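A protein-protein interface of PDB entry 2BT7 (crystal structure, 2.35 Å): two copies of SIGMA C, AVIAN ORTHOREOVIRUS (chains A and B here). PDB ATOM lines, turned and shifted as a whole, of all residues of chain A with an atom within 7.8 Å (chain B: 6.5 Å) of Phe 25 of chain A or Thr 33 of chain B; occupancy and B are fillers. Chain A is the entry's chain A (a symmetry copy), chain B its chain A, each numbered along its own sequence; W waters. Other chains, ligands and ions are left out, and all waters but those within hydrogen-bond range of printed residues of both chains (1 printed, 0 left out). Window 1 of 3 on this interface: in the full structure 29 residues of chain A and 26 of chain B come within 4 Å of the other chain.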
ATOM      1  N   PRO A   9      -6.013   8.399 -29.286  1.00  0.00           N
ATOM      2  CA  PRO A   9      -5.289   9.435 -30.052  1.00  0.00           C
ATOM      3  C   PRO A   9      -5.774   9.675 -31.510  1.00  0.00           C
ATOM      4  O   PRO A   9      -5.158  10.458 -32.252  1.00  0.00           O
ATOM      5  CB  PRO A   9      -3.850   8.911 -30.046  1.00  0.00           C
ATOM      6  CG  PRO A   9      -4.028   7.389 -30.035  1.00  0.00           C
ATOM      7  CD  PRO A   9      -5.373   7.074 -29.419  1.00  0.00           C
ATOM      8  N   LEU A  19      -3.997  10.634 -36.696  1.00  0.00           N
ATOM      9  CA  LEU A  19      -3.402  10.105 -35.475  1.00  0.00           C
ATOM     10  C   LEU A  19      -2.535  11.223 -34.924  1.00  0.00           C
ATOM     11  O   LEU A  19      -1.572  11.645 -35.569  1.00  0.00           O
ATOM     12  CB  LEU A  19      -2.591   8.834 -35.744  1.00  0.00           C
ATOM     13  CG  LEU A  19      -1.740   8.228 -34.611  1.00  0.00           C
ATOM     14  CD1 LEU A  19      -2.580   7.633 -33.479  1.00  0.00           C
ATOM     15  CD2 LEU A  19      -0.735   7.180 -35.149  1.00  0.00           C
ATOM     16  N   ASP A  20      -2.925  11.728 -33.751  1.00  0.00           N
ATOM     17  CA  ASP A  20      -2.086  12.637 -32.977  1.00  0.00           C
ATOM     18  C   ASP A  20      -0.866  11.900 -32.394  1.00  0.00           C
ATOM     19  O   ASP A  20      -1.004  10.894 -31.701  1.00  0.00           O
ATOM     20  CB  ASP A  20      -2.914  13.340 -31.902  1.00  0.00           C
ATOM     21  CG  ASP A  20      -4.109  14.114 -32.506  1.00  0.00           C
ATOM     22  OD1 ASP A  20      -3.913  14.844 -33.510  1.00  0.00           O
ATOM     23  OD2 ASP A  20      -5.244  13.967 -32.003  1.00  0.00           O
ATOM     24  N   MET A  21       0.322  12.400 -32.718  1.00  0.00           N
ATOM     25  CA  MET A  21       1.571  11.738 -32.342  1.00  0.00           C
ATOM     26  C   MET A  21       2.429  12.588 -31.407  1.00  0.00           C
ATOM     27  O   MET A  21       2.645  13.766 -31.665  1.00  0.00           O
ATOM     28  CB  MET A  21       2.343  11.364 -33.598  1.00  0.00           C
ATOM     29  CG  MET A  21       1.703  10.222 -34.343  1.00  0.00           C
ATOM     30  SD  MET A  21       2.231  10.055 -36.052  1.00  0.00           S
ATOM     31  CE  MET A  21       1.794  11.663 -36.711  1.00  0.00           C
ATOM     32  N   ASP A  22       2.848  12.013 -30.284  1.00  0.00           N
ATOM     33  CA  ASP A  22       3.896  12.596 -29.432  1.00  0.00           C
ATOM     34  C   ASP A  22       5.171  12.500 -30.229  1.00  0.00           C
ATOM     35  O   ASP A  22       5.614  11.395 -30.531  1.00  0.00           O
ATOM     36  CB  ASP A  22       4.027  11.733 -28.175  1.00  0.00           C
ATOM     37  CG  ASP A  22       5.114  12.216 -27.204  1.00  0.00           C
ATOM     38  OD1 ASP A  22       5.724  13.294 -27.417  1.00  0.00           O
ATOM     39  OD2 ASP A  22       5.325  11.479 -26.209  1.00  0.00           O
ATOM     40  N   PRO A  23       5.741  13.643 -30.652  1.00  0.00           N
ATOM     41  CA  PRO A  23       6.963  13.542 -31.471  1.00  0.00           C
ATOM     42  C   PRO A  23       8.215  12.971 -30.729  1.00  0.00           C
ATOM     43  O   PRO A  23       9.143  12.508 -31.392  1.00  0.00           O
ATOM     44  CB  PRO A  23       7.203  14.984 -31.911  1.00  0.00           C
ATOM     45  CG  PRO A  23       6.589  15.798 -30.850  1.00  0.00           C
ATOM     46  CD  PRO A  23       5.341  15.044 -30.463  1.00  0.00           C
ATOM     47  N   TYR A  24       8.226  13.003 -29.390  1.00  0.00           N
ATOM     48  CA  TYR A  24       9.268  12.341 -28.582  1.00  0.00           C
ATOM     49  C   TYR A  24       9.134  10.840 -28.614  1.00  0.00           C
ATOM     50  O   TYR A  24      10.049  10.135 -28.207  1.00  0.00           O
ATOM     51  CB  TYR A  24       9.264  12.848 -27.122  1.00  0.00           C
ATOM     52  CG  TYR A  24       9.718  14.272 -27.064  1.00  0.00           C
ATOM     53  CD1 TYR A  24      11.081  14.583 -27.038  1.00  0.00           C
ATOM     54  CD2 TYR A  24       8.799  15.322 -27.123  1.00  0.00           C
ATOM     55  CE1 TYR A  24      11.529  15.919 -27.037  1.00  0.00           C
ATOM     56  CE2 TYR A  24       9.226  16.654 -27.118  1.00  0.00           C
ATOM     57  CZ  TYR A  24      10.588  16.943 -27.075  1.00  0.00           C
ATOM     58  OH  TYR A  24      11.010  18.251 -27.073  1.00  0.00           O
ATOM     59  N   PHE A  25       7.986  10.353 -29.082  1.00  0.00           N
ATOM     60  CA  PHE A  25       7.734   8.908 -29.171  1.00  0.00           C
ATOM     61  C   PHE A  25       7.566   8.394 -30.601  1.00  0.00           C
ATOM     62  O   PHE A  25       8.140   7.364 -30.965  1.00  0.00           O
ATOM     63  CB  PHE A  25       6.531   8.505 -28.333  1.00  0.00           C
ATOM     64  CG  PHE A  25       6.225   7.040 -28.398  1.00  0.00           C
ATOM     65  CD1 PHE A  25       7.121   6.100 -27.874  1.00  0.00           C
ATOM     66  CD2 PHE A  25       5.033   6.586 -28.980  1.00  0.00           C
ATOM     67  CE1 PHE A  25       6.824   4.712 -27.920  1.00  0.00           C
ATOM     68  CE2 PHE A  25       4.726   5.202 -29.035  1.00  0.00           C
ATOM     69  CZ  PHE A  25       5.632   4.267 -28.506  1.00  0.00           C
ATOM     70  N   CYS A  26       6.790   9.114 -31.412  1.00  0.00           N
ATOM     71  CA  CYS A  26       6.510   8.666 -32.767  1.00  0.00           C
ATOM     72  C   CYS A  26       6.325   9.795 -33.786  1.00  0.00           C
ATOM     73  O   CYS A  26       6.208  10.961 -33.447  1.00  0.00           O
ATOM     74  CB  CYS A  26       5.340   7.662 -32.797  1.00  0.00           C
ATOM     75  SG  CYS A  26       3.709   8.290 -32.105  1.00  0.00           S
ATOM     76  N   SER A  27       6.322   9.403 -35.053  1.00  0.00           N
ATOM     77  CA  SER A  27       6.154  10.288 -36.155  1.00  0.00           C
ATOM     78  C   SER A  27       5.586   9.410 -37.287  1.00  0.00           C
ATOM     79  O   SER A  27       5.400   8.195 -37.100  1.00  0.00           O
ATOM     80  CB  SER A  27       7.512  10.878 -36.545  1.00  0.00           C
ATOM     81  OG  SER A  27       8.380   9.843 -36.984  1.00  0.00           O
ATOM     82  N   LEU A  32       3.763   4.490 -39.486  1.00  0.00           N
ATOM     83  CA  LEU A  32       4.004   4.944 -38.121  1.00  0.00           C
ATOM     84  C   LEU A  32       5.378   4.428 -37.682  1.00  0.00           C
ATOM     85  O   LEU A  32       5.652   3.222 -37.735  1.00  0.00           O
ATOM     86  CB  LEU A  32       2.904   4.456 -37.166  1.00  0.00           C
ATOM     87  CG  LEU A  32       3.086   4.811 -35.676  1.00  0.00           C
ATOM     88  CD1 LEU A  32       3.015   6.308 -35.376  1.00  0.00           C
ATOM     89  CD2 LEU A  32       2.110   4.049 -34.823  1.00  0.00           C
ATOM     90  N   THR A  33       6.232   5.360 -37.276  1.00  0.00           N
ATOM     91  CA  THR A  33       7.632   5.055 -36.974  1.00  0.00           C
ATOM     92  C   THR A  33       8.097   5.734 -35.664  1.00  0.00           C
ATOM     93  O   THR A  33       7.273   6.300 -34.918  1.00  0.00           O
ATOM     94  CB  THR A  33       8.521   5.354 -38.201  1.00  0.00           C
ATOM     95  OG1 THR A  33       9.823   4.764 -38.038  1.00  0.00           O
ATOM     96  CG2 THR A  33       8.606   6.842 -38.475  1.00  0.00           C
ATOM     97  N   SER A  34       9.403   5.679 -35.381  1.00  0.00           N
ATOM     98  CA  SER A  34       9.960   6.218 -34.119  1.00  0.00           C
ATOM     99  C   SER A  34       9.960   7.742 -34.093  1.00  0.00           C
ATOM    100  O   SER A  34       9.595   8.374 -35.067  1.00  0.00           O
ATOM    101  CB  SER A  34      11.374   5.642 -33.834  1.00  0.00           C
ATOM    102  OG  SER A  34      12.208   5.792 -34.983  1.00  0.00           O
ATOM    103  N   TYR A  35      10.395   8.314 -32.972  1.00  0.00           N
ATOM    104  CA  TYR A  35      10.372   9.740 -32.698  1.00  0.00           C
ATOM    105  C   TYR A  35      11.090  10.605 -33.719  1.00  0.00           C
ATOM    106  O   TYR A  35      12.082  10.189 -34.334  1.00  0.00           O
ATOM    107  CB  TYR A  35      10.927  10.014 -31.282  1.00  0.00           C
ATOM    108  CG  TYR A  35      12.423   9.823 -31.159  1.00  0.00           C
ATOM    109  CD1 TYR A  35      12.965   8.552 -30.887  1.00  0.00           C
ATOM    110  CD2 TYR A  35      13.294  10.898 -31.328  1.00  0.00           C
ATOM    111  CE1 TYR A  35      14.330   8.360 -30.813  1.00  0.00           C
ATOM    112  CE2 TYR A  35      14.689  10.715 -31.257  1.00  0.00           C
ATOM    113  CZ  TYR A  35      15.193   9.438 -31.002  1.00  0.00           C
ATOM    114  OH  TYR A  35      16.547   9.234 -30.897  1.00  0.00           O
ATOM    115  N   SER A  36      10.600  11.841 -33.847  1.00  0.00           N
ATOM    116  CA  SER A  36      11.134  12.812 -34.776  1.00  0.00           C
ATOM    117  C   SER A  36      11.786  13.977 -34.016  1.00  0.00           C
ATOM    118  O   SER A  36      12.543  14.765 -34.605  1.00  0.00           O
ATOM    119  CB  SER A  36      10.001  13.360 -35.677  1.00  0.00           C
ATOM    120  OG  SER A  36       8.964  13.933 -34.895  1.00  0.00           O
ATOM    121  N   ALA A  37      11.470  14.102 -32.728  1.00  0.00           N
ATOM    122  CA  ALA A  37      12.073  15.138 -31.893  1.00  0.00           C
ATOM    123  C   ALA A  37      13.591  15.008 -31.862  1.00  0.00           C
ATOM    124  O   ALA A  37      14.128  13.903 -31.808  1.00  0.00           O
ATOM    125  CB  ALA A  37      11.524  15.088 -30.488  1.00  0.00           C
ATOM    126  N   HIS A  67      16.971  11.137 -25.758  1.00  0.00           N
ATOM    127  CA  HIS A  67      16.774  10.579 -27.073  1.00  0.00           C
ATOM    128  C   HIS A  67      15.437   9.835 -27.086  1.00  0.00           C
ATOM    129  O   HIS A  67      15.237   8.789 -26.420  1.00  0.00           O
ATOM    130  CB  HIS A  67      17.994   9.718 -27.512  1.00  0.00           C
ATOM    131  CG  HIS A  67      18.305   8.581 -26.588  1.00  0.00           C
ATOM    132  ND1 HIS A  67      18.188   7.255 -26.972  1.00  0.00           N
ATOM    133  CD2 HIS A  67      18.704   8.567 -25.291  1.00  0.00           C
ATOM    134  CE1 HIS A  67      18.492   6.475 -25.947  1.00  0.00           C
ATOM    135  NE2 HIS A  67      18.806   7.246 -24.915  1.00  0.00           N
ATOM    136  N   GLY A  68      14.487  10.404 -27.820  1.00  0.00           N
ATOM    137  CA  GLY A  68      13.098   9.969 -27.686  1.00  0.00           C
ATOM    138  C   GLY A  68      12.680  10.280 -26.264  1.00  0.00           C
ATOM    139  O   GLY A  68      12.973  11.357 -25.762  1.00  0.00           O
ATOM    140  N   ARG A  69      12.016   9.332 -25.612  1.00  0.00           N
ATOM    141  CA  ARG A  69      11.571   9.494 -24.234  1.00  0.00           C
ATOM    142  C   ARG A  69      12.514   8.729 -23.255  1.00  0.00           C
ATOM    143  O   ARG A  69      12.138   8.391 -22.116  1.00  0.00           O
ATOM    144  CB  ARG A  69      10.088   9.040 -24.084  1.00  0.00           C
ATOM    145  CG  ARG A  69       9.075   9.797 -24.972  1.00  0.00           C
ATOM    146  CD  ARG A  69       7.638   9.739 -24.447  1.00  0.00           C
ATOM    147  NE  ARG A  69       7.494  10.532 -23.226  1.00  0.00           N
ATOM    148  CZ  ARG A  69       7.203  11.832 -23.169  1.00  0.00           C
ATOM    149  NH1 ARG A  69       6.980  12.546 -24.270  1.00  0.00           N
ATOM    150  NH2 ARG A  69       7.151  12.434 -21.986  1.00  0.00           N
ATOM    151  N   ARG A 106      12.300  16.416 -19.839  1.00  0.00           N
ATOM    152  CA  ARG A 106      13.241  15.329 -20.106  1.00  0.00           C
ATOM    153  C   ARG A 106      13.894  14.721 -18.851  1.00  0.00           C
ATOM    154  O   ARG A 106      14.570  13.706 -18.948  1.00  0.00           O
ATOM    155  CB  ARG A 106      14.322  15.774 -21.080  1.00  0.00           C
ATOM    156  CG  ARG A 106      13.797  16.450 -22.337  1.00  0.00           C
ATOM    157  CD  ARG A 106      13.375  15.478 -23.427  1.00  0.00           C
ATOM    158  NE  ARG A 106      12.380  14.489 -23.026  1.00  0.00           N
ATOM    159  CZ  ARG A 106      11.069  14.700 -22.999  1.00  0.00           C
ATOM    160  NH1 ARG A 106      10.581  15.892 -23.325  1.00  0.00           N
ATOM    161  NH2 ARG A 106      10.241  13.711 -22.649  1.00  0.00           N
ATOM    162  N   THR A 170      10.925   8.663 -19.751  1.00  0.00           N
ATOM    163  CA  THR A 170      10.189   9.887 -19.422  1.00  0.00           C
ATOM    164  C   THR A 170       8.787   9.893 -20.072  1.00  0.00           C
ATOM    165  O   THR A 170       8.439   8.979 -20.830  1.00  0.00           O
ATOM    166  CB  THR A 170      10.962  11.155 -19.865  1.00  0.00           C
ATOM    167  OG1 THR A 170      11.048  11.173 -21.292  1.00  0.00           O
ATOM    168  CG2 THR A 170      12.405  11.190 -19.268  1.00  0.00           C
ATOM    169  OXT THR A 170       7.966  10.801 -19.852  1.00  0.00           O
ATOM    170  N   MET B  21      -4.395  -0.078 -27.853  1.00  0.00           N
ATOM    171  CA  MET B  21      -3.004   0.126 -27.452  1.00  0.00           C
ATOM    172  C   MET B  21      -2.519  -0.925 -26.456  1.00  0.00           C
ATOM    173  O   MET B  21      -3.195  -1.206 -25.475  1.00  0.00           O
ATOM    174  CB  MET B  21      -2.841   1.528 -26.886  1.00  0.00           C
ATOM    175  CG  MET B  21      -2.921   2.589 -27.952  1.00  0.00           C
ATOM    176  SD  MET B  21      -3.250   4.243 -27.337  1.00  0.00           S
ATOM    177  CE  MET B  21      -4.798   3.994 -26.470  1.00  0.00           C
ATOM    178  N   PHE B  25       3.548  -0.911 -24.337  1.00  0.00           N
ATOM    179  CA  PHE B  25       4.203  -0.211 -25.450  1.00  0.00           C
ATOM    180  C   PHE B  25       3.748   1.238 -25.626  1.00  0.00           C
ATOM    181  O   PHE B  25       4.576   2.134 -25.811  1.00  0.00           O
ATOM    182  CB  PHE B  25       4.028  -0.968 -26.758  1.00  0.00           C
ATOM    183  CG  PHE B  25       4.670  -0.289 -27.929  1.00  0.00           C
ATOM    184  CD1 PHE B  25       6.062  -0.149 -27.996  1.00  0.00           C
ATOM    185  CD2 PHE B  25       3.888   0.212 -28.979  1.00  0.00           C
ATOM    186  CE1 PHE B  25       6.672   0.481 -29.114  1.00  0.00           C
ATOM    187  CE2 PHE B  25       4.485   0.845 -30.098  1.00  0.00           C
ATOM    188  CZ  PHE B  25       5.883   0.981 -30.157  1.00  0.00           C
ATOM    189  N   CYS B  26       2.436   1.469 -25.558  1.00  0.00           N
ATOM    190  CA  CYS B  26       1.902   2.803 -25.786  1.00  0.00           C
ATOM    191  C   CYS B  26       0.643   3.132 -24.977  1.00  0.00           C
ATOM    192  O   CYS B  26       0.024   2.277 -24.365  1.00  0.00           O
ATOM    193  CB  CYS B  26       1.714   3.084 -27.290  1.00  0.00           C
ATOM    194  SG  CYS B  26       0.575   1.900 -28.203  1.00  0.00           S
ATOM    195  N   SER B  27       0.299   4.413 -24.985  1.00  0.00           N
ATOM    196  CA  SER B  27      -0.841   4.930 -24.307  1.00  0.00           C
ATOM    197  C   SER B  27      -1.207   6.217 -25.072  1.00  0.00           C
ATOM    198  O   SER B  27      -0.521   6.584 -26.042  1.00  0.00           O
ATOM    199  CB  SER B  27      -0.472   5.239 -22.854  1.00  0.00           C
ATOM    200  OG  SER B  27       0.519   6.256 -22.814  1.00  0.00           O
ATOM    201  N   GLN B  28      -2.295   6.879 -24.668  1.00  0.00           N
ATOM    202  CA  GLN B  28      -2.552   8.218 -25.172  1.00  0.00           C
ATOM    203  C   GLN B  28      -2.633   9.141 -24.005  1.00  0.00           C
ATOM    204  O   GLN B  28      -3.226   8.809 -22.996  1.00  0.00           O
ATOM    205  CB  GLN B  28      -3.835   8.316 -26.037  1.00  0.00           C
ATOM    206  CG  GLN B  28      -5.188   7.952 -25.345  1.00  0.00           C
ATOM    207  CD  GLN B  28      -5.800   9.099 -24.532  1.00  0.00           C
ATOM    208  OE1 GLN B  28      -5.518  10.265 -24.785  1.00  0.00           O
ATOM    209  NE2 GLN B  28      -6.642   8.755 -23.535  1.00  0.00           N
ATOM    210  N   ARG B  29      -2.007  10.288 -24.131  1.00  0.00           N
ATOM    211  CA  ARG B  29      -2.300  11.383 -23.252  1.00  0.00           C
ATOM    212  C   ARG B  29      -2.609  12.486 -24.279  1.00  0.00           C
ATOM    213  O   ARG B  29      -1.771  13.353 -24.556  1.00  0.00           O
ATOM    214  CB  ARG B  29      -1.096  11.700 -22.326  1.00  0.00           C
ATOM    215  CG  ARG B  29      -0.355  10.439 -21.796  1.00  0.00           C
ATOM    216  CD  ARG B  29      -0.155  10.398 -20.268  1.00  0.00           C
ATOM    217  NE  ARG B  29       0.095   9.027 -19.772  1.00  0.00           N
ATOM    218  CZ  ARG B  29       0.383   8.690 -18.504  1.00  0.00           C
ATOM    219  NH1 ARG B  29       0.464   9.616 -17.551  1.00  0.00           N
ATOM    220  NH2 ARG B  29       0.596   7.412 -18.178  1.00  0.00           N
ATOM    221  N   SER B  31      -2.169  12.841 -27.487  1.00  0.00           N
ATOM    222  CA  SER B  31      -1.351  12.237 -28.555  1.00  0.00           C
ATOM    223  C   SER B  31      -0.874  10.842 -28.179  1.00  0.00           C
ATOM    224  O   SER B  31      -0.913  10.453 -27.005  1.00  0.00           O
ATOM    225  CB  SER B  31      -0.161  13.110 -28.892  1.00  0.00           C
ATOM    226  OG  SER B  31       0.398  13.622 -27.710  1.00  0.00           O
ATOM    227  N   LEU B  32      -0.478  10.075 -29.190  1.00  0.00           N
ATOM    228  CA  LEU B  32       0.031   8.723 -28.988  1.00  0.00           C
ATOM    229  C   LEU B  32       1.447   8.827 -28.413  1.00  0.00           C
ATOM    230  O   LEU B  32       2.323   9.481 -28.993  1.00  0.00           O
ATOM    231  CB  LEU B  32       0.028   7.922 -30.298  1.00  0.00           C
ATOM    232  CG  LEU B  32       0.614   6.497 -30.228  1.00  0.00           C
ATOM    233  CD1 LEU B  32      -0.189   5.531 -29.359  1.00  0.00           C
ATOM    234  CD2 LEU B  32       0.812   5.933 -31.609  1.00  0.00           C
ATOM    235  N   THR B  33       1.640   8.197 -27.260  1.00  0.00           N
ATOM    236  CA  THR B  33       2.886   8.327 -26.501  1.00  0.00           C
ATOM    237  C   THR B  33       3.384   6.959 -25.977  1.00  0.00           C
ATOM    238  O   THR B  33       2.840   5.902 -26.354  1.00  0.00           O
ATOM    239  CB  THR B  33       2.737   9.414 -25.413  1.00  0.00           C
ATOM    240  OG1 THR B  33       4.025   9.779 -24.884  1.00  0.00           O
ATOM    241  CG2 THR B  33       1.782   8.979 -24.321  1.00  0.00           C
ATOM    242  N   SER B  34       4.409   6.974 -25.119  1.00  0.00           N
ATOM    243  CA  SER B  34       5.029   5.729 -24.610  1.00  0.00           C
ATOM    244  C   SER B  34       4.132   5.001 -23.615  1.00  0.00           C
ATOM    245  O   SER B  34       3.071   5.488 -23.274  1.00  0.00           O
ATOM    246  CB  SER B  34       6.438   6.003 -24.014  1.00  0.00           C
ATOM    247  OG  SER B  34       6.378   7.080 -23.081  1.00  0.00           O
ATOM    248  N   TYR B  35       4.589   3.842 -23.146  1.00  0.00           N
ATOM    249  CA  TYR B  35       3.847   2.940 -22.282  1.00  0.00           C
ATOM    250  C   TYR B  35       3.342   3.556 -20.989  1.00  0.00           C
ATOM    251  O   TYR B  35       3.966   4.460 -20.418  1.00  0.00           O
ATOM    252  CB  TYR B  35       4.694   1.685 -21.981  1.00  0.00           C
ATOM    253  CG  TYR B  35       5.854   1.933 -21.040  1.00  0.00           C
ATOM    254  CD1 TYR B  35       7.094   2.383 -21.533  1.00  0.00           C
ATOM    255  CD2 TYR B  35       5.711   1.740 -19.667  1.00  0.00           C
ATOM    256  CE1 TYR B  35       8.145   2.653 -20.679  1.00  0.00           C
ATOM    257  CE2 TYR B  35       6.776   2.013 -18.786  1.00  0.00           C
ATOM    258  CZ  TYR B  35       7.987   2.473 -19.306  1.00  0.00           C
ATOM    259  OH  TYR B  35       9.051   2.719 -18.475  1.00  0.00           O
HETATM  260  O   HOH W   1       8.668   6.633 -21.525  1.00  0.00           O
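The side-chain hydroxyl (OG1) of Thr 33 of chain B sits at hydrogen-bond distance from the side-chain carboxylate (OD2) of Asp 22 of chain A (2.5 Å).
The backbone NH (N) of Leu 32 of chain B lies within hydrogen-bond range of the backbone carbonyl oxygen (O) of Asp 20 of chain A, 2.7 Å away.
The backbone carbonyl oxygen of Leu 32 of chain B sits at hydrogen-bond distance from the backbone NH of Asp 22 of chain A, at 2.9 Å.
The backbone carbonyl oxygen of Leu 32 of chain B is in hydrogen-bond range of the side-chain sulfur of Cys 26 of chain A.
The side-chain hydroxyl (OG) of Ser 27 of chain B sits at hydrogen-bond distance from the backbone carbonyl oxygen (O) of Ser 34 of chain B (2.7 Å).
The backbone carbonyl oxygen (O) of Phe 25 of chain A is in hydrogen-bond range of the backbone NH (N) of Tyr 35 of chain A (3.2 Å).
The backbone carbonyl oxygen (O) of Phe 25 of chain B is in hydrogen-bond range of the backbone NH (N) of Tyr 35 of chain B (3.2 Å).
The backbone NH (N) of Asp 20 of chain A lies within hydrogen-bond range of the backbone carbonyl oxygen (O) of Pro 9 of chain A (3.0 Å).
The side-chain carboxylate of Asp 22 of chain A is in hydrogen-bond range of the backbone NH of Tyr 24 of chain A, at 3.2 Å.
O of Tyr 24 of chain A lies within hydrogen-bond range of N of Arg 69 of chain A (3.4 Å).
Pro 9 of chain A touches Leu 32 of chain B (CB to N, 3.7 Å).
CA of Ser 31 of chain B touches O of Asp 20 of chain A, at 3.4 Å.
Ser 31 of chain B touches Met 21 of chain A (CB to C, 3.6 Å).
Met 21 of chain A touches Leu 32 of chain B (C to O, 3.9 Å).
Asp 22 of chain A touches Ser 31 of chain B (N to CB, 3.5 Å).
Phe 25 of chain A touches Phe 25 of chain B.
CD2 of Phe 25 of chain A touches O of Leu 32 of chain B, 3.97 Å away.
Thr 33 of chain B touches Phe 25 of chain A.
CD2 of Leu 32 of chain B touches CD2 of Leu 32 of chain A (3.9 Å).
OG of Ser 34 of chain B touches CD of Arg 69 of chain A, 3.2 Å away.
Of the printed residues of chain B, Pro 9 of chain A touches Gln 28 and Leu 32.
Of the printed residues of chain B, Asp 20 of chain A touches Ser 31 and Leu 32.
Of chain B, only Phe 25 (3.6 Å), Leu 32 (3.97 Å), Thr 33 (3.4 Å) and Ser 34 (3.7 Å) come within 4 Å of Phe 25 of chain A.
Of the printed residues of chain B, Cys 26 of chain A touches Leu 32.
Printed residues of chain A within 4 Å of Leu 32 of chain B: Pro 9, Asp 20, Met 21, Asp 22, Phe 25, Cys 26 and Leu 32.
Thr 33 of chain B touches just these residues of chain A: Asp 22 (2.5 Å), Phe 25 (3.4 Å) and Arg 69 (3.6 Å).
Of the printed residues of chain A, Ser 34 of chain B touches Phe 25 (3.7 Å), Arg 69 (3.2 Å) and Thr 170 (3.6 Å).
The nearest residue of chain B that does not touch Phe 25 of chain A is Cys 26 of chain B (4.1 Å).
Hydrophobic or aromatic side chains of chain A within 4 Å of the printed part of chain B: Pro 9, Phe 25 and Leu 32.
Of the 11 printed residues of chain B, 6 touch a printed residue of chain A.
Printed residues of chain B that touch a printed residue of chain A: Phe 25, Gln 28, Ser 31, Leu 32, Thr 33 and Ser 34.
Hydrophobic or aromatic side chains of chain B that line the printed part of chain A: Phe 25 and Leu 32.
Among the printed residues, no Asp or Glu carboxylate lies within 4 Å of a Lys or Arg side-chain nitrogen of the other chain.
Phe 25 of chain A touches Leu 32 of chain B, but with the chains exchanged Leu 32 of chain A does not touch Phe 25 of chain B (6.2 Å).
Phe 25 of chain A touches Thr 33 of chain B, but with the chains exchanged Thr 33 of chain A does not touch Phe 25 of chain B (7.3 Å).
Cys 26 of chain A touches Leu 32 of chain B, but with the chains exchanged Leu 32 of chain A does not touch Cys 26 of chain B (7.1 Å).
Leu 32 of chain A touches its own counterpart, Leu 32 of chain B.
8 positions are printed for both chains.
Of the 18 pairs that touch across the chains among the printed residues, 2 have their exchanged pair printed and touching as well.
Water W1 bridges the chain-end carboxylate of Thr 170 of chain A (2.5 Å) and the side-chain hydroxyl of Ser 34 of chain B (2.8 Å).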
